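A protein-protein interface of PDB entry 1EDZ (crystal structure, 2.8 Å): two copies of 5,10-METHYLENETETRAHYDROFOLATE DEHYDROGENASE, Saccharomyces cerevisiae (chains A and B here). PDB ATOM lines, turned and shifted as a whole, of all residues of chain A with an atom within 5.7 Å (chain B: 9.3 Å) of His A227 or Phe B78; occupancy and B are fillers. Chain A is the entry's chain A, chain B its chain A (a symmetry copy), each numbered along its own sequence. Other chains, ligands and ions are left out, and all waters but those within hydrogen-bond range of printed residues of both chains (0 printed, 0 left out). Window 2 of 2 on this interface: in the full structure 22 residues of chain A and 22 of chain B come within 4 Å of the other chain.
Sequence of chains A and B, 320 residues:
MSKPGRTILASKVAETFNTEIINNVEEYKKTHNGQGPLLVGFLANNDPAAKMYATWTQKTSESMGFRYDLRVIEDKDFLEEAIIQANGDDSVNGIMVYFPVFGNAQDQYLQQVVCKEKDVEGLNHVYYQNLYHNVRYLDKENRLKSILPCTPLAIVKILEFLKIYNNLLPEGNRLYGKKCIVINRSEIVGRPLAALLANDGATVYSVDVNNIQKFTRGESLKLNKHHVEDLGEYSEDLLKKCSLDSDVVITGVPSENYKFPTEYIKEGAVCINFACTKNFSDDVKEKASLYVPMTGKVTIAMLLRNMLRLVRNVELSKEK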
ATOM      1  N   LYS A 214     -25.585  -7.782 -36.441  1.00  0.00           N
ATOM      2  CA  LYS A 214     -26.035  -9.039 -35.858  1.00  0.00           C
ATOM      3  C   LYS A 214     -25.827  -9.078 -34.352  1.00  0.00           C
ATOM      4  O   LYS A 214     -24.713  -9.256 -33.863  1.00  0.00           O
ATOM      5  CB  LYS A 214     -25.322 -10.209 -36.539  1.00  0.00           C
ATOM      6  CG  LYS A 214     -25.626 -11.578 -35.959  1.00  0.00           C
ATOM      7  CD  LYS A 214     -25.061 -12.675 -36.861  1.00  0.00           C
ATOM      8  CE  LYS A 214     -24.766 -13.955 -36.090  1.00  0.00           C
ATOM      9  NZ  LYS A 214     -23.615 -13.776 -35.163  1.00  0.00           N
ATOM     10  N   PHE A 215     -26.914  -8.881 -33.619  1.00  0.00           N
ATOM     11  CA  PHE A 215     -26.869  -8.893 -32.168  1.00  0.00           C
ATOM     12  C   PHE A 215     -26.947 -10.326 -31.673  1.00  0.00           C
ATOM     13  O   PHE A 215     -27.785 -11.104 -32.135  1.00  0.00           O
ATOM     14  CB  PHE A 215     -28.026  -8.074 -31.591  1.00  0.00           C
ATOM     15  CG  PHE A 215     -27.905  -6.593 -31.830  1.00  0.00           C
ATOM     16  CD1 PHE A 215     -27.010  -6.090 -32.770  1.00  0.00           C
ATOM     17  CD2 PHE A 215     -28.681  -5.696 -31.103  1.00  0.00           C
ATOM     18  CE1 PHE A 215     -26.889  -4.718 -32.982  1.00  0.00           C
ATOM     19  CE2 PHE A 215     -28.567  -4.320 -31.307  1.00  0.00           C
ATOM     20  CZ  PHE A 215     -27.668  -3.831 -32.248  1.00  0.00           C
ATOM     21  N   THR A 216     -26.064 -10.670 -30.744  1.00  0.00           N
ATOM     22  CA  THR A 216     -26.012 -12.007 -30.169  1.00  0.00           C
ATOM     23  C   THR A 216     -25.781 -11.891 -28.668  1.00  0.00           C
ATOM     24  O   THR A 216     -25.649 -10.784 -28.142  1.00  0.00           O
ATOM     25  CB  THR A 216     -24.864 -12.828 -30.789  1.00  0.00           C
ATOM     26  OG1 THR A 216     -23.656 -12.055 -30.776  1.00  0.00           O
ATOM     27  CG2 THR A 216     -25.198 -13.220 -32.222  1.00  0.00           C
ATOM     28  N   ARG A 217     -25.719 -13.030 -27.983  1.00  0.00           N
ATOM     29  CA  ARG A 217     -25.486 -13.050 -26.541  1.00  0.00           C
ATOM     30  C   ARG A 217     -24.180 -12.323 -26.197  1.00  0.00           C
ATOM     31  O   ARG A 217     -23.244 -12.296 -27.002  1.00  0.00           O
ATOM     32  CB  ARG A 217     -25.411 -14.490 -26.042  1.00  0.00           C
ATOM     33  CG  ARG A 217     -25.344 -14.622 -24.533  1.00  0.00           C
ATOM     34  CD  ARG A 217     -26.726 -14.586 -23.913  1.00  0.00           C
ATOM     35  NE  ARG A 217     -27.519 -15.754 -24.297  1.00  0.00           N
ATOM     36  CZ  ARG A 217     -28.597 -16.174 -23.642  1.00  0.00           C
ATOM     37  NH1 ARG A 217     -29.014 -15.523 -22.562  1.00  0.00           N
ATOM     38  NH2 ARG A 217     -29.266 -17.233 -24.074  1.00  0.00           N
ATOM     39  N   GLY A 218     -24.127 -11.738 -25.004  1.00  0.00           N
ATOM     40  CA  GLY A 218     -22.946 -11.013 -24.572  1.00  0.00           C
ATOM     41  C   GLY A 218     -21.674 -11.836 -24.495  1.00  0.00           C
ATOM     42  O   GLY A 218     -21.661 -12.930 -23.925  1.00  0.00           O
ATOM     43  N   GLU A 219     -20.600 -11.292 -25.060  1.00  0.00           N
ATOM     44  CA  GLU A 219     -19.301 -11.954 -25.069  1.00  0.00           C
ATOM     45  C   GLU A 219     -18.344 -11.252 -24.121  1.00  0.00           C
ATOM     46  O   GLU A 219     -17.195 -10.982 -24.477  1.00  0.00           O
ATOM     47  CB  GLU A 219     -18.703 -11.934 -26.482  1.00  0.00           C
ATOM     48  CG  GLU A 219     -19.299 -12.942 -27.442  1.00  0.00           C
ATOM     49  CD  GLU A 219     -19.149 -14.366 -26.956  1.00  0.00           C
ATOM     50  OE1 GLU A 219     -18.087 -14.725 -26.398  1.00  0.00           O
ATOM     51  OE2 GLU A 219     -20.108 -15.145 -27.109  1.00  0.00           O
ATOM     52  N   SER A 220     -18.799 -10.953 -22.913  1.00  0.00           N
ATOM     53  CA  SER A 220     -17.942 -10.263 -21.965  1.00  0.00           C
ATOM     54  C   SER A 220     -18.246 -10.536 -20.500  1.00  0.00           C
ATOM     55  O   SER A 220     -19.374 -10.864 -20.132  1.00  0.00           O
ATOM     56  CB  SER A 220     -17.998  -8.759 -22.223  1.00  0.00           C
ATOM     57  OG  SER A 220     -17.401  -8.055 -21.156  1.00  0.00           O
ATOM     58  N   LYS A 225     -24.019  -7.303 -21.429  1.00  0.00           N
ATOM     59  CA  LYS A 225     -24.724  -6.622 -22.508  1.00  0.00           C
ATOM     60  C   LYS A 225     -24.583  -7.389 -23.816  1.00  0.00           C
ATOM     61  O   LYS A 225     -23.507  -7.877 -24.144  1.00  0.00           O
ATOM     62  CB  LYS A 225     -24.147  -5.213 -22.676  1.00  0.00           C
ATOM     63  CG  LYS A 225     -24.552  -4.500 -23.954  1.00  0.00           C
ATOM     64  CD  LYS A 225     -23.677  -3.281 -24.178  1.00  0.00           C
ATOM     65  CE  LYS A 225     -23.947  -2.649 -25.529  1.00  0.00           C
ATOM     66  NZ  LYS A 225     -23.042  -1.499 -25.800  1.00  0.00           N
ATOM     67  N   HIS A 226     -25.680  -7.490 -24.559  1.00  0.00           N
ATOM     68  CA  HIS A 226     -25.691  -8.181 -25.845  1.00  0.00           C
ATOM     69  C   HIS A 226     -24.463  -7.814 -26.675  1.00  0.00           C
ATOM     70  O   HIS A 226     -24.086  -6.639 -26.765  1.00  0.00           O
ATOM     71  CB  HIS A 226     -26.930  -7.775 -26.634  1.00  0.00           C
ATOM     72  CG  HIS A 226     -26.900  -6.353 -27.102  1.00  0.00           C
ATOM     73  ND1 HIS A 226     -27.076  -5.283 -26.248  1.00  0.00           N
ATOM     74  CD2 HIS A 226     -26.680  -5.824 -28.327  1.00  0.00           C
ATOM     75  CE1 HIS A 226     -26.965  -4.156 -26.929  1.00  0.00           C
ATOM     76  NE2 HIS A 226     -26.726  -4.457 -28.193  1.00  0.00           N
ATOM     77  N   HIS A 227     -23.847  -8.812 -27.292  1.00  0.00           N
ATOM     78  CA  HIS A 227     -22.680  -8.560 -28.120  1.00  0.00           C
ATOM     79  C   HIS A 227     -23.150  -8.120 -29.499  1.00  0.00           C
ATOM     80  O   HIS A 227     -23.990  -8.775 -30.116  1.00  0.00           O
ATOM     81  CB  HIS A 227     -21.805  -9.812 -28.235  1.00  0.00           C
ATOM     82  CG  HIS A 227     -20.560  -9.602 -29.038  1.00  0.00           C
ATOM     83  ND1 HIS A 227     -20.386 -10.139 -30.296  1.00  0.00           N
ATOM     84  CD2 HIS A 227     -19.443  -8.880 -28.780  1.00  0.00           C
ATOM     85  CE1 HIS A 227     -19.218  -9.755 -30.780  1.00  0.00           C
ATOM     86  NE2 HIS A 227     -18.628  -8.989 -29.879  1.00  0.00           N
ATOM     87  N   VAL A 228     -22.625  -6.998 -29.970  1.00  0.00           N
ATOM     88  CA  VAL A 228     -23.000  -6.483 -31.277  1.00  0.00           C
ATOM     89  C   VAL A 228     -21.999  -6.877 -32.357  1.00  0.00           C
ATOM     90  O   VAL A 228     -20.859  -6.407 -32.370  1.00  0.00           O
ATOM     91  CB  VAL A 228     -23.140  -4.945 -31.258  1.00  0.00           C
ATOM     92  CG1 VAL A 228     -23.380  -4.416 -32.661  1.00  0.00           C
ATOM     93  CG2 VAL A 228     -24.276  -4.534 -30.338  1.00  0.00           C
ATOM     94  N   GLU A 229     -22.400  -7.803 -33.213  1.00  0.00           N
ATOM     95  CA  GLU A 229     -21.538  -8.213 -34.306  1.00  0.00           C
ATOM     96  C   GLU A 229     -21.939  -7.286 -35.452  1.00  0.00           C
ATOM     97  O   GLU A 229     -23.110  -6.906 -35.568  1.00  0.00           O
ATOM     98  CB  GLU A 229     -21.784  -9.675 -34.673  1.00  0.00           C
ATOM     99  CG  GLU A 229     -20.788 -10.236 -35.677  1.00  0.00           C
ATOM    100  CD  GLU A 229     -21.122 -11.653 -36.103  1.00  0.00           C
ATOM    101  OE1 GLU A 229     -21.402 -12.491 -35.218  1.00  0.00           O
ATOM    102  OE2 GLU A 229     -21.120 -11.934 -37.320  1.00  0.00           O
ATOM    103  N   PHE B  42     -12.029   9.559 -23.912  1.00  0.00           N
ATOM    104  CA  PHE B  42     -12.466   8.409 -24.693  1.00  0.00           C
ATOM    105  C   PHE B  42     -12.502   8.678 -26.178  1.00  0.00           C
ATOM    106  O   PHE B  42     -13.338   9.442 -26.664  1.00  0.00           O
ATOM    107  CB  PHE B  42     -13.825   7.908 -24.204  1.00  0.00           C
ATOM    108  CG  PHE B  42     -13.746   7.114 -22.937  1.00  0.00           C
ATOM    109  CD1 PHE B  42     -14.116   7.676 -21.726  1.00  0.00           C
ATOM    110  CD2 PHE B  42     -13.273   5.811 -22.951  1.00  0.00           C
ATOM    111  CE1 PHE B  42     -14.014   6.948 -20.548  1.00  0.00           C
ATOM    112  CE2 PHE B  42     -13.167   5.076 -21.780  1.00  0.00           C
ATOM    113  CZ  PHE B  42     -13.538   5.645 -20.575  1.00  0.00           C
ATOM    114  N   LEU B  43     -11.574   8.053 -26.892  1.00  0.00           N
ATOM    115  CA  LEU B  43     -11.475   8.203 -28.331  1.00  0.00           C
ATOM    116  C   LEU B  43     -12.022   6.910 -28.902  1.00  0.00           C
ATOM    117  O   LEU B  43     -11.685   5.833 -28.416  1.00  0.00           O
ATOM    118  CB  LEU B  43     -10.010   8.384 -28.726  1.00  0.00           C
ATOM    119  CG  LEU B  43      -9.686   9.068 -30.054  1.00  0.00           C
ATOM    120  CD1 LEU B  43     -10.115   8.211 -31.236  1.00  0.00           C
ATOM    121  CD2 LEU B  43     -10.357  10.431 -30.088  1.00  0.00           C
ATOM    122  N   ALA B  44     -12.873   7.005 -29.917  1.00  0.00           N
ATOM    123  CA  ALA B  44     -13.454   5.806 -30.511  1.00  0.00           C
ATOM    124  C   ALA B  44     -13.916   6.045 -31.934  1.00  0.00           C
ATOM    125  O   ALA B  44     -14.789   5.337 -32.445  1.00  0.00           O
ATOM    126  CB  ALA B  44     -14.613   5.309 -29.655  1.00  0.00           C
ATOM    127  N   ARG B  71      -7.903   6.801 -23.224  1.00  0.00           N
ATOM    128  CA  ARG B  71      -8.265   5.455 -23.624  1.00  0.00           C
ATOM    129  C   ARG B  71      -8.865   5.404 -25.025  1.00  0.00           C
ATOM    130  O   ARG B  71      -9.900   6.010 -25.295  1.00  0.00           O
ATOM    131  CB  ARG B  71      -9.163   4.841 -22.544  1.00  0.00           C
ATOM    132  CG  ARG B  71      -8.470   4.948 -21.184  1.00  0.00           C
ATOM    133  CD  ARG B  71      -9.235   4.435 -19.975  1.00  0.00           C
ATOM    134  NE  ARG B  71      -8.486   4.796 -18.769  1.00  0.00           N
ATOM    135  CZ  ARG B  71      -8.933   4.697 -17.519  1.00  0.00           C
ATOM    136  NH1 ARG B  71     -10.151   4.228 -17.269  1.00  0.00           N
ATOM    137  NH2 ARG B  71      -8.168   5.110 -16.515  1.00  0.00           N
ATOM    138  N   VAL B  72      -8.160   4.732 -25.929  1.00  0.00           N
ATOM    139  CA  VAL B  72      -8.590   4.593 -27.320  1.00  0.00           C
ATOM    140  C   VAL B  72      -9.253   3.243 -27.536  1.00  0.00           C
ATOM    141  O   VAL B  72      -8.617   2.209 -27.365  1.00  0.00           O
ATOM    142  CB  VAL B  72      -7.392   4.689 -28.288  1.00  0.00           C
ATOM    143  CG1 VAL B  72      -7.876   4.638 -29.734  1.00  0.00           C
ATOM    144  CG2 VAL B  72      -6.585   5.955 -28.010  1.00  0.00           C
ATOM    145  N   ILE B  73     -10.524   3.257 -27.921  1.00  0.00           N
ATOM    146  CA  ILE B  73     -11.281   2.026 -28.158  1.00  0.00           C
ATOM    147  C   ILE B  73     -11.225   1.652 -29.633  1.00  0.00           C
ATOM    148  O   ILE B  73     -11.176   2.531 -30.494  1.00  0.00           O
ATOM    149  CB  ILE B  73     -12.762   2.178 -27.724  1.00  0.00           C
ATOM    150  CG1 ILE B  73     -12.868   2.250 -26.200  1.00  0.00           C
ATOM    151  CG2 ILE B  73     -13.592   1.010 -28.216  1.00  0.00           C
ATOM    152  CD1 ILE B  73     -12.304   3.513 -25.590  1.00  0.00           C
ATOM    153  N   GLU B  74     -11.208   0.351 -29.920  1.00  0.00           N
ATOM    154  CA  GLU B  74     -11.161  -0.127 -31.297  1.00  0.00           C
ATOM    155  C   GLU B  74     -12.559  -0.032 -31.919  1.00  0.00           C
ATOM    156  O   GLU B  74     -12.830   0.881 -32.706  1.00  0.00           O
ATOM    157  CB  GLU B  74     -10.626  -1.561 -31.351  1.00  0.00           C
ATOM    158  CG  GLU B  74     -10.233  -2.029 -32.749  1.00  0.00           C
ATOM    159  CD  GLU B  74      -9.409  -3.311 -32.748  1.00  0.00           C
ATOM    160  OE1 GLU B  74      -9.545  -4.124 -31.807  1.00  0.00           O
ATOM    161  OE2 GLU B  74      -8.620  -3.510 -33.700  1.00  0.00           O
ATOM    162  N   ASP B  75     -13.446  -0.957 -31.564  1.00  0.00           N
ATOM    163  CA  ASP B  75     -14.811  -0.929 -32.081  1.00  0.00           C
ATOM    164  C   ASP B  75     -15.743  -0.223 -31.099  1.00  0.00           C
ATOM    165  O   ASP B  75     -15.689  -0.438 -29.884  1.00  0.00           O
ATOM    166  CB  ASP B  75     -15.322  -2.334 -32.428  1.00  0.00           C
ATOM    167  CG  ASP B  75     -14.785  -3.395 -31.498  1.00  0.00           C
ATOM    168  OD1 ASP B  75     -14.673  -3.121 -30.286  1.00  0.00           O
ATOM    169  OD2 ASP B  75     -14.459  -4.495 -31.985  1.00  0.00           O
ATOM    170  N   LYS B  76     -16.605   0.620 -31.656  1.00  0.00           N
ATOM    171  CA  LYS B  76     -17.548   1.427 -30.898  1.00  0.00           C
ATOM    172  C   LYS B  76     -18.376   0.722 -29.830  1.00  0.00           C
ATOM    173  O   LYS B  76     -18.533   1.235 -28.720  1.00  0.00           O
ATOM    174  CB  LYS B  76     -18.477   2.175 -31.858  1.00  0.00           C
ATOM    175  CG  LYS B  76     -17.771   3.160 -32.779  1.00  0.00           C
ATOM    176  CD  LYS B  76     -17.293   2.516 -34.078  1.00  0.00           C
ATOM    177  CE  LYS B  76     -16.449   3.486 -34.910  1.00  0.00           C
ATOM    178  NZ  LYS B  76     -17.105   4.818 -35.092  1.00  0.00           N
ATOM    179  N   ASP B  77     -18.873  -0.465 -30.141  1.00  0.00           N
ATOM    180  CA  ASP B  77     -19.715  -1.198 -29.203  1.00  0.00           C
ATOM    181  C   ASP B  77     -19.160  -1.469 -27.815  1.00  0.00           C
ATOM    182  O   ASP B  77     -19.931  -1.669 -26.867  1.00  0.00           O
ATOM    183  CB  ASP B  77     -20.223  -2.480 -29.846  1.00  0.00           C
ATOM    184  CG  ASP B  77     -21.159  -2.199 -30.991  1.00  0.00           C
ATOM    185  OD1 ASP B  77     -22.350  -1.923 -30.734  1.00  0.00           O
ATOM    186  OD2 ASP B  77     -20.692  -2.200 -32.146  1.00  0.00           O
ATOM    187  N   PHE B  78     -17.838  -1.466 -27.676  1.00  0.00           N
ATOM    188  CA  PHE B  78     -17.239  -1.708 -26.372  1.00  0.00           C
ATOM    189  C   PHE B  78     -16.933  -0.421 -25.621  1.00  0.00           C
ATOM    190  O   PHE B  78     -16.528  -0.461 -24.463  1.00  0.00           O
ATOM    191  CB  PHE B  78     -16.003  -2.596 -26.498  1.00  0.00           C
ATOM    192  CG  PHE B  78     -16.322  -4.022 -26.858  1.00  0.00           C
ATOM    193  CD1 PHE B  78     -16.286  -4.448 -28.180  1.00  0.00           C
ATOM    194  CD2 PHE B  78     -16.679  -4.937 -25.874  1.00  0.00           C
ATOM    195  CE1 PHE B  78     -16.599  -5.764 -28.522  1.00  0.00           C
ATOM    196  CE2 PHE B  78     -16.996  -6.254 -26.203  1.00  0.00           C
ATOM    197  CZ  PHE B  78     -16.955  -6.668 -27.531  1.00  0.00           C
ATOM    198  N   LEU B  79     -17.185   0.718 -26.265  1.00  0.00           N
ATOM    199  CA  LEU B  79     -16.953   2.031 -25.655  1.00  0.00           C
ATOM    200  C   LEU B  79     -17.788   2.116 -24.389  1.00  0.00           C
ATOM    201  O   LEU B  79     -17.292   2.493 -23.324  1.00  0.00           O
ATOM    202  CB  LEU B  79     -17.405   3.152 -26.594  1.00  0.00           C
ATOM    203  CG  LEU B  79     -16.821   4.564 -26.444  1.00  0.00           C
ATOM    204  CD1 LEU B  79     -17.824   5.553 -26.985  1.00  0.00           C
ATOM    205  CD2 LEU B  79     -16.489   4.908 -25.006  1.00  0.00           C
ATOM    206  N   GLU B  80     -19.067   1.773 -24.527  1.00  0.00           N
ATOM    207  CA  GLU B  80     -20.003   1.799 -23.414  1.00  0.00           C
ATOM    208  C   GLU B  80     -19.378   1.101 -22.214  1.00  0.00           C
ATOM    209  O   GLU B  80     -19.134   1.728 -21.183  1.00  0.00           O
ATOM    210  CB  GLU B  80     -21.302   1.101 -23.815  1.00  0.00           C
ATOM    211  CG  GLU B  80     -22.463   1.302 -22.843  1.00  0.00           C
ATOM    212  CD  GLU B  80     -23.774   0.764 -23.382  1.00  0.00           C
ATOM    213  OE1 GLU B  80     -23.949   0.712 -24.618  1.00  0.00           O
ATOM    214  OE2 GLU B  80     -24.636   0.377 -22.574  1.00  0.00           O
ATOM    215  N   GLU B  81     -19.036  -0.170 -22.393  1.00  0.00           N
ATOM    216  CA  GLU B  81     -18.430  -0.979 -21.339  1.00  0.00           C
ATOM    217  C   GLU B  81     -17.300  -0.244 -20.632  1.00  0.00           C
ATOM    218  O   GLU B  81     -17.212  -0.241 -19.398  1.00  0.00           O
ATOM    219  CB  GLU B  81     -17.898  -2.279 -21.937  1.00  0.00           C
ATOM    220  CG  GLU B  81     -17.122  -3.148 -20.977  1.00  0.00           C
ATOM    221  CD  GLU B  81     -16.527  -4.353 -21.665  1.00  0.00           C
ATOM    222  OE1 GLU B  81     -15.524  -4.203 -22.392  1.00  0.00           O
ATOM    223  OE2 GLU B  81     -17.078  -5.453 -21.492  1.00  0.00           O
ATOM    224  N   ALA B  82     -16.457   0.406 -21.423  1.00  0.00           N
ATOM    225  CA  ALA B  82     -15.327   1.142 -20.887  1.00  0.00           C
ATOM    226  C   ALA B  82     -15.810   2.254 -19.971  1.00  0.00           C
ATOM    227  O   ALA B  82     -15.220   2.508 -18.915  1.00  0.00           O
ATOM    228  CB  ALA B  82     -14.488   1.710 -22.019  1.00  0.00           C
ATOM    229  N   ILE B  83     -16.909   2.889 -20.352  1.00  0.00           N
ATOM    230  CA  ILE B  83     -17.446   3.979 -19.562  1.00  0.00           C
ATOM    231  C   ILE B  83     -17.883   3.541 -18.169  1.00  0.00           C
ATOM    232  O   ILE B  83     -17.491   4.165 -17.182  1.00  0.00           O
ATOM    233  CB  ILE B  83     -18.591   4.702 -20.292  1.00  0.00           C
ATOM    234  CG1 ILE B  83     -18.099   5.195 -21.655  1.00  0.00           C
ATOM    235  CG2 ILE B  83     -19.071   5.888 -19.465  1.00  0.00           C
ATOM    236  CD1 ILE B  83     -19.139   5.920 -22.468  1.00  0.00           C
ATOM    237  N   ILE B  84     -18.652   2.458 -18.071  1.00  0.00           N
ATOM    238  CA  ILE B  84     -19.104   2.000 -16.754  1.00  0.00           C
ATOM    239  C   ILE B  84     -17.954   1.636 -15.827  1.00  0.00           C
ATOM    240  O   ILE B  84     -17.928   2.068 -14.668  1.00  0.00           O
ATOM    241  CB  ILE B  84     -20.102   0.812 -16.794  1.00  0.00           C
ATOM    242  CG1 ILE B  84     -20.052   0.073 -18.128  1.00  0.00           C
ATOM    243  CG2 ILE B  84     -21.507   1.310 -16.503  1.00  0.00           C
ATOM    244  CD1 ILE B  84     -20.922   0.687 -19.196  1.00  0.00           C
ATOM    245  N   GLN B  85     -16.984   0.880 -16.334  1.00  0.00           N
ATOM    246  CA  GLN B  85     -15.854   0.499 -15.498  1.00  0.00           C
ATOM    247  C   GLN B  85     -15.134   1.754 -14.998  1.00  0.00           C
ATOM    248  O   GLN B  85     -14.627   1.788 -13.878  1.00  0.00           O
ATOM    249  CB  GLN B  85     -14.906  -0.454 -16.240  1.00  0.00           C
ATOM    250  CG  GLN B  85     -14.092   0.162 -17.357  1.00  0.00           C
ATOM    251  CD  GLN B  85     -12.611   0.205 -17.033  1.00  0.00           C
ATOM    252  OE1 GLN B  85     -11.904  -0.800 -17.160  1.00  0.00           O
ATOM    253  NE2 GLN B  85     -12.130   1.369 -16.604  1.00  0.00           N
ATOM    254  N   VAL B 101     -18.994   9.129 -32.154  1.00  0.00           N
ATOM    255  CA  VAL B 101     -18.602   7.743 -31.960  1.00  0.00           C
ATOM    256  C   VAL B 101     -19.431   6.928 -32.948  1.00  0.00           C
ATOM    257  O   VAL B 101     -18.884   6.328 -33.882  1.00  0.00           O
ATOM    258  CB  VAL B 101     -18.868   7.269 -30.523  1.00  0.00           C
ATOM    259  CG1 VAL B 101     -18.454   5.808 -30.367  1.00  0.00           C
ATOM    260  CG2 VAL B 101     -18.117   8.156 -29.536  1.00  0.00           C
ATOM    261  N   PHE B 102     -20.747   6.921 -32.741  1.00  0.00           N
ATOM    262  CA  PHE B 102     -21.688   6.216 -33.615  1.00  0.00           C
ATOM    263  C   PHE B 102     -22.288   7.224 -34.594  1.00  0.00           C
ATOM    264  O   PHE B 102     -22.802   6.857 -35.654  1.00  0.00           O
ATOM    265  CB  PHE B 102     -22.817   5.574 -32.804  1.00  0.00           C
ATOM    266  CG  PHE B 102     -22.494   4.211 -32.269  1.00  0.00           C
ATOM    267  CD1 PHE B 102     -22.503   3.968 -30.897  1.00  0.00           C
ATOM    268  CD2 PHE B 102     -22.221   3.157 -33.134  1.00  0.00           C
ATOM    269  CE1 PHE B 102     -22.249   2.697 -30.396  1.00  0.00           C
ATOM    270  CE2 PHE B 102     -21.963   1.873 -32.642  1.00  0.00           C
ATOM    271  CZ  PHE B 102     -21.980   1.644 -31.269  1.00  0.00           C
ATOM    272  N   GLN B 106     -27.397   6.993 -30.752  1.00  0.00           N
ATOM    273  CA  GLN B 106     -26.530   6.260 -29.839  1.00  0.00           C
ATOM    274  C   GLN B 106     -25.576   7.174 -29.079  1.00  0.00           C
ATOM    275  O   GLN B 106     -25.301   6.944 -27.905  1.00  0.00           O
ATOM    276  CB  GLN B 106     -25.737   5.182 -30.572  1.00  0.00           C
ATOM    277  CG  GLN B 106     -26.539   3.954 -30.947  1.00  0.00           C
ATOM    278  CD  GLN B 106     -25.711   2.676 -30.856  1.00  0.00           C
ATOM    279  OE1 GLN B 106     -25.377   2.213 -29.763  1.00  0.00           O
ATOM    280  NE2 GLN B 106     -25.380   2.100 -32.005  1.00  0.00           N
ATOM    281  N   LEU B 110     -25.071   7.518 -25.272  1.00  0.00           N
ATOM    282  CA  LEU B 110     -23.763   7.391 -24.646  1.00  0.00           C
ATOM    283  C   LEU B 110     -23.500   8.537 -23.697  1.00  0.00           C
ATOM    284  O   LEU B 110     -23.043   8.317 -22.578  1.00  0.00           O
ATOM    285  CB  LEU B 110     -22.660   7.318 -25.701  1.00  0.00           C
ATOM    286  CG  LEU B 110     -22.604   6.018 -26.510  1.00  0.00           C
ATOM    287  CD1 LEU B 110     -21.597   6.141 -27.645  1.00  0.00           C
ATOM    288  CD2 LEU B 110     -22.261   4.850 -25.595  1.00  0.00           C
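The side-chain hydroxyl (OG) of Ser A220 lies within hydrogen-bond range of the side-chain carboxylate (OE2) of Glu B81 (2.6 Å). O of Asp B77 lies within hydrogen-bond range of NZ of Lys A225, 3.3 Å away. The side-chain amino group of Lys A225 is in salt-bridge range of the side-chain carboxylate of Glu B80, at 2.7 Å.
O of Thr A216 is in hydrogen-bond range of N of His A227 (2.8 Å).
CZ of Phe B78 touches CD2 of His A227, at 3.6 Å. Asp B77 touches Val A228 (OD1 to CB, 3.2 Å).
His A227 touches just one residue of chain B: Phe B78. Phe B78 touches one residue of chain A. No residue of chain B comes within 4 Å of Thr A216. Printed residues of chain B within 4 Å of Ser A220: Glu B81 (2.6 Å). Of the printed residues of chain A, Asp B77 touches Lys A225 and Val A228. Of the printed residues of chain B, Lys A225 touches Asp B77 and Glu B80. Printed residues of chain A within 4 Å of Glu B80: Lys A225 (2.7 Å). Ile B84 touches none of the printed residues of chain A. Phe B102 touches none of the printed residues of chain A. The nearest residue of chain B that does not touch His A227 is Asp B77 (6.4 Å).
Hydrophobic or aromatic side chains of chain A that line the printed part of chain B: His A227 and Val A228. Hydrophobic or aromatic side chains of chain B that line the printed part of chain A: Phe B78. Along chain B the printed residues that touch a printed residue of chain A span positions 77 to 81. Among the printed residues, 5 pairs touch across the chains. Among the printed residues, Asp or Glu carboxylates within 4 Å of a Lys or Arg side-chain nitrogen of the other chain: Lys A225 with Glu B80.
No position is printed for both chains.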
